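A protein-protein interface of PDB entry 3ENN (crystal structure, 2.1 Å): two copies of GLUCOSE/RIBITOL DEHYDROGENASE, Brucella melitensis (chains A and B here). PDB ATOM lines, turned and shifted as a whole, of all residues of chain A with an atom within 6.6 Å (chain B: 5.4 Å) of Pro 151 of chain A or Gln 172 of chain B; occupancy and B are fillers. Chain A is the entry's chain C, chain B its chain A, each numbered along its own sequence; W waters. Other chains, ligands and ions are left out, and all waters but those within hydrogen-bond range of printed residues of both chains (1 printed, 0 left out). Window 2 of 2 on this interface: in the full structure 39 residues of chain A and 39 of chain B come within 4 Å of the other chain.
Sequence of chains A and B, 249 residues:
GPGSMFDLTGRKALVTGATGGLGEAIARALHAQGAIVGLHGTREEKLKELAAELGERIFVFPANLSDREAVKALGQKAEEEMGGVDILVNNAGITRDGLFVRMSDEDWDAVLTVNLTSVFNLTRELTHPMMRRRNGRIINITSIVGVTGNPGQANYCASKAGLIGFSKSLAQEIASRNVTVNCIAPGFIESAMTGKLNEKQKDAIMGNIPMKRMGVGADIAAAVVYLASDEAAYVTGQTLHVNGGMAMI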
ATOM      1  N   ASP A  97     -22.224 -20.709   9.315  1.00  0.00           N
ATOM      2  CA  ASP A  97     -21.017 -20.372  10.035  1.00  0.00           C
ATOM      3  C   ASP A  97     -21.221 -20.530  11.519  1.00  0.00           C
ATOM      4  O   ASP A  97     -22.332 -20.366  12.020  1.00  0.00           O
ATOM      5  CB  ASP A  97     -20.584 -18.935   9.721  1.00  0.00           C
ATOM      6  CG  ASP A  97     -20.111 -18.764   8.288  1.00  0.00           C
ATOM      7  OD1 ASP A  97     -20.037 -19.770   7.525  1.00  0.00           O
ATOM      8  OD2 ASP A  97     -19.807 -17.611   7.921  1.00  0.00           O
ATOM      9  N   GLY A  98     -20.136 -20.865  12.203  1.00  0.00           N
ATOM     10  CA  GLY A  98     -20.117 -20.938  13.652  1.00  0.00           C
ATOM     11  C   GLY A  98     -18.913 -21.726  14.103  1.00  0.00           C
ATOM     12  O   GLY A  98     -18.266 -22.423  13.303  1.00  0.00           O
ATOM     13  N   LEU A  99     -18.609 -21.631  15.392  1.00  0.00           N
ATOM     14  CA  LEU A  99     -17.519 -22.412  15.959  1.00  0.00           C
ATOM     15  C   LEU A  99     -17.742 -23.877  15.673  1.00  0.00           C
ATOM     16  O   LEU A  99     -18.866 -24.358  15.732  1.00  0.00           O
ATOM     17  CB  LEU A  99     -17.387 -22.184  17.471  1.00  0.00           C
ATOM     18  CG  LEU A  99     -16.770 -20.881  18.019  1.00  0.00           C
ATOM     19  CD1 LEU A  99     -16.132 -19.982  16.925  1.00  0.00           C
ATOM     20  CD2 LEU A  99     -17.791 -20.134  18.871  1.00  0.00           C
ATOM     21  N   THR A 148      -7.555 -21.648   1.809  1.00  0.00           N
ATOM     22  CA  THR A 148      -6.845 -21.056   2.962  1.00  0.00           C
ATOM     23  C   THR A 148      -7.279 -21.626   4.302  1.00  0.00           C
ATOM     24  O   THR A 148      -6.518 -21.627   5.269  1.00  0.00           O
ATOM     25  CB  THR A 148      -6.994 -19.502   3.034  1.00  0.00           C
ATOM     26  OG1 THR A 148      -8.379 -19.122   3.192  1.00  0.00           O
ATOM     27  CG2 THR A 148      -6.420 -18.848   1.788  1.00  0.00           C
ATOM     28  N   GLY A 149      -8.519 -22.092   4.347  1.00  0.00           N
ATOM     29  CA  GLY A 149      -9.204 -22.310   5.587  1.00  0.00           C
ATOM     30  C   GLY A 149      -9.722 -20.970   6.093  1.00  0.00           C
ATOM     31  O   GLY A 149      -9.305 -19.891   5.648  1.00  0.00           O
ATOM     32  N   ASN A 150     -10.647 -21.061   7.035  1.00  0.00           N
ATOM     33  CA  ASN A 150     -11.207 -19.896   7.695  1.00  0.00           C
ATOM     34  C   ASN A 150     -11.891 -20.408   8.936  1.00  0.00           C
ATOM     35  O   ASN A 150     -12.714 -21.333   8.833  1.00  0.00           O
ATOM     36  CB  ASN A 150     -12.252 -19.200   6.806  1.00  0.00           C
ATOM     37  CG  ASN A 150     -12.528 -17.766   7.226  1.00  0.00           C
ATOM     38  OD1 ASN A 150     -11.655 -17.072   7.741  1.00  0.00           O
ATOM     39  ND2 ASN A 150     -13.740 -17.307   6.965  1.00  0.00           N
ATOM     40  N   PRO A 151     -11.578 -19.803  10.102  1.00  0.00           N
ATOM     41  CA  PRO A 151     -12.282 -20.229  11.300  1.00  0.00           C
ATOM     42  C   PRO A 151     -13.767 -19.940  11.160  1.00  0.00           C
ATOM     43  O   PRO A 151     -14.161 -18.998  10.451  1.00  0.00           O
ATOM     44  CB  PRO A 151     -11.670 -19.378  12.422  1.00  0.00           C
ATOM     45  CG  PRO A 151     -10.930 -18.274  11.768  1.00  0.00           C
ATOM     46  CD  PRO A 151     -10.603 -18.726  10.368  1.00  0.00           C
ATOM     47  N   GLY A 152     -14.575 -20.771  11.801  1.00  0.00           N
ATOM     48  CA  GLY A 152     -16.001 -20.532  11.878  1.00  0.00           C
ATOM     49  C   GLY A 152     -16.692 -21.108  10.669  1.00  0.00           C
ATOM     50  O   GLY A 152     -17.914 -20.995  10.541  1.00  0.00           O
ATOM     51  N   GLN A 153     -15.901 -21.708   9.772  1.00  0.00           N
ATOM     52  CA  GLN A 153     -16.426 -22.299   8.532  1.00  0.00           C
ATOM     53  C   GLN A 153     -15.875 -23.688   8.221  1.00  0.00           C
ATOM     54  O   GLN A 153     -15.593 -23.993   7.064  1.00  0.00           O
ATOM     55  CB  GLN A 153     -16.133 -21.386   7.347  1.00  0.00           C
ATOM     56  CG  GLN A 153     -16.628 -19.980   7.518  1.00  0.00           C
ATOM     57  CD  GLN A 153     -16.633 -19.243   6.216  1.00  0.00           C
ATOM     58  OE1 GLN A 153     -15.583 -18.932   5.657  1.00  0.00           O
ATOM     59  NE2 GLN A 153     -17.824 -18.952   5.720  1.00  0.00           N
ATOM     60  N   ALA A 154     -15.713 -24.524   9.239  1.00  0.00           N
ATOM     61  CA  ALA A 154     -15.278 -25.911   9.003  1.00  0.00           C
ATOM     62  C   ALA A 154     -16.096 -26.562   7.874  1.00  0.00           C
ATOM     63  O   ALA A 154     -15.546 -27.208   6.974  1.00  0.00           O
ATOM     64  CB  ALA A 154     -15.387 -26.713  10.267  1.00  0.00           C
ATOM     65  N   CYS A 157     -15.611 -24.450   4.262  1.00  0.00           N
ATOM     66  CA  CYS A 157     -14.279 -24.777   3.742  1.00  0.00           C
ATOM     67  C   CYS A 157     -14.150 -26.228   3.249  1.00  0.00           C
ATOM     68  O   CYS A 157     -13.524 -26.474   2.216  1.00  0.00           O
ATOM     69  CB  CYS A 157     -13.191 -24.490   4.794  1.00  0.00           C
ATOM     70  SG  CYS A 157     -13.078 -22.764   5.264  1.00  0.00           S
ATOM     71  N   SER B 167      -9.837 -29.509   7.549  1.00  0.00           N
ATOM     72  CA  SER B 167      -8.708 -29.488   8.429  1.00  0.00           C
ATOM     73  C   SER B 167      -8.114 -28.097   8.582  1.00  0.00           C
ATOM     74  O   SER B 167      -7.734 -27.712   9.689  1.00  0.00           O
ATOM     75  CB  SER B 167      -7.630 -30.462   7.947  1.00  0.00           C
ATOM     76  OG  SER B 167      -8.146 -31.795   7.896  1.00  0.00           O
ATOM     77  N   LYS B 168      -7.996 -27.371   7.468  1.00  0.00           N
ATOM     78  CA  LYS B 168      -7.418 -26.035   7.487  1.00  0.00           C
ATOM     79  C   LYS B 168      -8.292 -25.098   8.306  1.00  0.00           C
ATOM     80  O   LYS B 168      -7.783 -24.329   9.099  1.00  0.00           O
ATOM     81  CB  LYS B 168      -7.230 -25.484   6.077  1.00  0.00           C
ATOM     82  CG  LYS B 168      -6.227 -26.234   5.250  1.00  0.00           C
ATOM     83  CD  LYS B 168      -6.173 -25.641   3.841  1.00  0.00           C
ATOM     84  CE  LYS B 168      -4.996 -26.219   3.042  1.00  0.00           C
ATOM     85  NZ  LYS B 168      -5.151 -25.982   1.549  1.00  0.00           N
ATOM     86  N   SER B 169      -9.609 -25.190   8.126  1.00  0.00           N
ATOM     87  CA  SER B 169     -10.518 -24.348   8.876  1.00  0.00           C
ATOM     88  C   SER B 169     -10.436 -24.642  10.365  1.00  0.00           C
ATOM     89  O   SER B 169     -10.359 -23.731  11.171  1.00  0.00           O
ATOM     90  CB  SER B 169     -11.937 -24.535   8.388  1.00  0.00           C
ATOM     91  OG  SER B 169     -12.832 -23.879   9.259  1.00  0.00           O
ATOM     92  N   LEU B 170     -10.450 -25.919  10.714  1.00  0.00           N
ATOM     93  CA  LEU B 170     -10.411 -26.328  12.103  1.00  0.00           C
ATOM     94  C   LEU B 170      -9.076 -25.939  12.713  1.00  0.00           C
ATOM     95  O   LEU B 170      -9.026 -25.398  13.812  1.00  0.00           O
ATOM     96  CB  LEU B 170     -10.684 -27.831  12.246  1.00  0.00           C
ATOM     97  CG  LEU B 170     -10.749 -28.350  13.686  1.00  0.00           C
ATOM     98  CD1 LEU B 170     -11.827 -27.605  14.484  1.00  0.00           C
ATOM     99  CD2 LEU B 170     -10.967 -29.858  13.686  1.00  0.00           C
ATOM    100  N   ALA B 171      -8.001 -26.189  11.971  1.00  0.00           N
ATOM    101  CA  ALA B 171      -6.676 -25.763  12.374  1.00  0.00           C
ATOM    102  C   ALA B 171      -6.655 -24.289  12.790  1.00  0.00           C
ATOM    103  O   ALA B 171      -6.123 -23.956  13.858  1.00  0.00           O
ATOM    104  CB  ALA B 171      -5.666 -26.017  11.272  1.00  0.00           C
ATOM    105  N   GLN B 172      -7.193 -23.419  11.938  1.00  0.00           N
ATOM    106  CA  GLN B 172      -7.209 -21.974  12.212  1.00  0.00           C
ATOM    107  C   GLN B 172      -7.964 -21.669  13.513  1.00  0.00           C
ATOM    108  O   GLN B 172      -7.561 -20.834  14.337  1.00  0.00           O
ATOM    109  CB  GLN B 172      -7.826 -21.231  11.027  1.00  0.00           C
ATOM    110  CG  GLN B 172      -6.819 -21.098   9.913  1.00  0.00           C
ATOM    111  CD  GLN B 172      -7.197 -20.137   8.848  1.00  0.00           C
ATOM    112  OE1 GLN B 172      -7.900 -19.150   9.084  1.00  0.00           O
ATOM    113  NE2 GLN B 172      -6.721 -20.402   7.644  1.00  0.00           N
ATOM    114  N   GLU B 173      -9.018 -22.434  13.721  1.00  0.00           N
ATOM    115  CA  GLU B 173      -9.922 -22.181  14.806  1.00  0.00           C
ATOM    116  C   GLU B 173      -9.366 -22.563  16.172  1.00  0.00           C
ATOM    117  O   GLU B 173      -9.624 -21.888  17.149  1.00  0.00           O
ATOM    118  CB  GLU B 173     -11.213 -22.920  14.524  1.00  0.00           C
ATOM    119  CG  GLU B 173     -12.443 -22.104  14.675  1.00  0.00           C
ATOM    120  CD  GLU B 173     -13.672 -22.903  14.367  1.00  0.00           C
ATOM    121  OE1 GLU B 173     -14.085 -22.905  13.209  1.00  0.00           O
ATOM    122  OE2 GLU B 173     -14.222 -23.533  15.285  1.00  0.00           O
ATOM    123  N   ILE B 174      -8.610 -23.653  16.244  1.00  0.00           N
ATOM    124  CA  ILE B 174      -8.243 -24.229  17.531  1.00  0.00           C
ATOM    125  C   ILE B 174      -6.733 -24.157  17.786  1.00  0.00           C
ATOM    126  O   ILE B 174      -6.259 -24.621  18.816  1.00  0.00           O
ATOM    127  CB  ILE B 174      -8.793 -25.676  17.670  1.00  0.00           C
ATOM    128  CG1 ILE B 174      -8.043 -26.643  16.752  1.00  0.00           C
ATOM    129  CG2 ILE B 174     -10.301 -25.705  17.382  1.00  0.00           C
ATOM    130  CD1 ILE B 174      -8.622 -28.052  16.718  1.00  0.00           C
ATOM    131  N   ALA B 175      -6.000 -23.538  16.858  1.00  0.00           N
ATOM    132  CA  ALA B 175      -4.534 -23.435  16.940  1.00  0.00           C
ATOM    133  C   ALA B 175      -4.045 -22.794  18.231  1.00  0.00           C
ATOM    134  O   ALA B 175      -3.087 -23.271  18.827  1.00  0.00           O
ATOM    135  CB  ALA B 175      -3.950 -22.674  15.723  1.00  0.00           C
ATOM    136  N   SER B 176      -4.713 -21.718  18.646  1.00  0.00           N
ATOM    137  CA  SER B 176      -4.331 -20.976  19.847  1.00  0.00           C
ATOM    138  C   SER B 176      -4.621 -21.769  21.131  1.00  0.00           C
ATOM    139  O   SER B 176      -4.199 -21.378  22.224  1.00  0.00           O
ATOM    140  CB  SER B 176      -5.016 -19.608  19.885  1.00  0.00           C
ATOM    141  OG  SER B 176      -6.377 -19.727  20.278  1.00  0.00           O
HETATM  142  O   HOH W   1     -16.198 -24.007  12.069  1.00  0.00           O
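OE2 of Glu 173 of chain B touches CA of Leu 99 of chain A, at 3.5 Å.
Gly 149 of chain A touches Lys 168 of chain B.
Ser 169 of chain B touches Gly 149 of chain A.
Asn 150 of chain A touches Gln 172 of chain B.
Pro 151 of chain A touches Ser 169 of chain B (CA to O, 3.997 Å).
OE1 of Gln 172 of chain B touches CD of Pro 151 of chain A, at 3.0 Å.
OE1 of Glu 173 of chain B touches C of Pro 151 of chain A, at 3.6 Å.
Gln 153 of chain A touches Ser 169 of chain B (C to OG, 3.2 Å).
Ser 169 of chain B touches Cys 157 of chain A (CB to SG, 3.8 Å).
Of the 10 printed residues of chain B, 4 touch a printed residue of chain A.
Printed residues of chain B that touch a printed residue of chain A: Lys 168, Ser 169, Gln 172 and Glu 173.
Of the 11 printed residues of chain A, 9 touch a printed residue of chain B.
Hydrophobic or aromatic side chains of chain A within 4 Å of the printed part of chain B: Pro 151 and Ala 154.
Among the printed residues, 14 pairs touch across the chains.
Among the printed residues, no Asp or Glu carboxylate lies within 4 Å of a Lys or Arg side-chain nitrogen of the other chain.
Printed residues of chain B within 4 Å of Thr 148 of chain A: Gln 172.
Of the printed residues of chain B, Asn 150 of chain A touches Ser 169 (2.6 Å) and Gln 172 (3.7 Å).
Printed residues of chain B within 4 Å of Pro 151 of chain A: Ser 169, Gln 172 and Glu 173.
Printed residues of chain B within 4 Å of Cys 157 of chain A: Ser 169.
Leu 170 of chain B touches none of the printed residues of chain A.
The nearest printed residue of chain B that does not touch Pro 151 of chain A is Lys 168 of chain B (6.0 Å).
The nearest printed residue of chain B that does not touch Ala 154 of chain A is Glu 173 of chain B (4.6 Å).
No position is printed for both chains.
NE2 of Gln 172 of chain B is in hydrogen-bond range of O of Thr 148 of chain A (2.7 Å).
The side-chain carboxylate (OE1) of Glu 173 of chain B lies within hydrogen-bond range of the backbone NH (N) of Gly 152 of chain A, 2.6 Å away.
OG of Ser 169 of chain B is in hydrogen-bond range of N of Ala 154 of chain A, 3.0 Å away.
OG of Ser 169 of chain B is in hydrogen-bond range of O of Asn 150 of chain A (2.6 Å).
The side-chain amide nitrogen (NE2) of Gln 172 of chain B is in hydrogen-bond range of the backbone carbonyl oxygen (O) of Gly 149 of chain A, 3.3 Å away.
Water W1 lies within hydrogen-bond range of OE1 of Glu 173 of chain B, O of Gly 98 of chain A, N of Ala 154 of chain A and N of Gln 153 of chain A.
N of Asn 150 of chain A lies within hydrogen-bond range of SG of Cys 157 of chain A.
The side-chain amide oxygen (OE1) of Gln 153 of chain A lies within hydrogen-bond range of the side-chain amide nitrogen (ND2) of Asn 150 of chain A (2.8 Å).
The backbone NH of Gly 98 of chain A sits at hydrogen-bond distance from the backbone carbonyl oxygen of Gly 152 of chain A, 2.8 Å away.
The backbone carbonyl oxygen of Gln 153 of chain A lies within hydrogen-bond range of the side-chain sulfur of Cys 157 of chain A (3.3 Å).
NE2 of Gln 153 of chain A sits at hydrogen-bond distance from OD1 of Asp 97 of chain A (3.0 Å).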
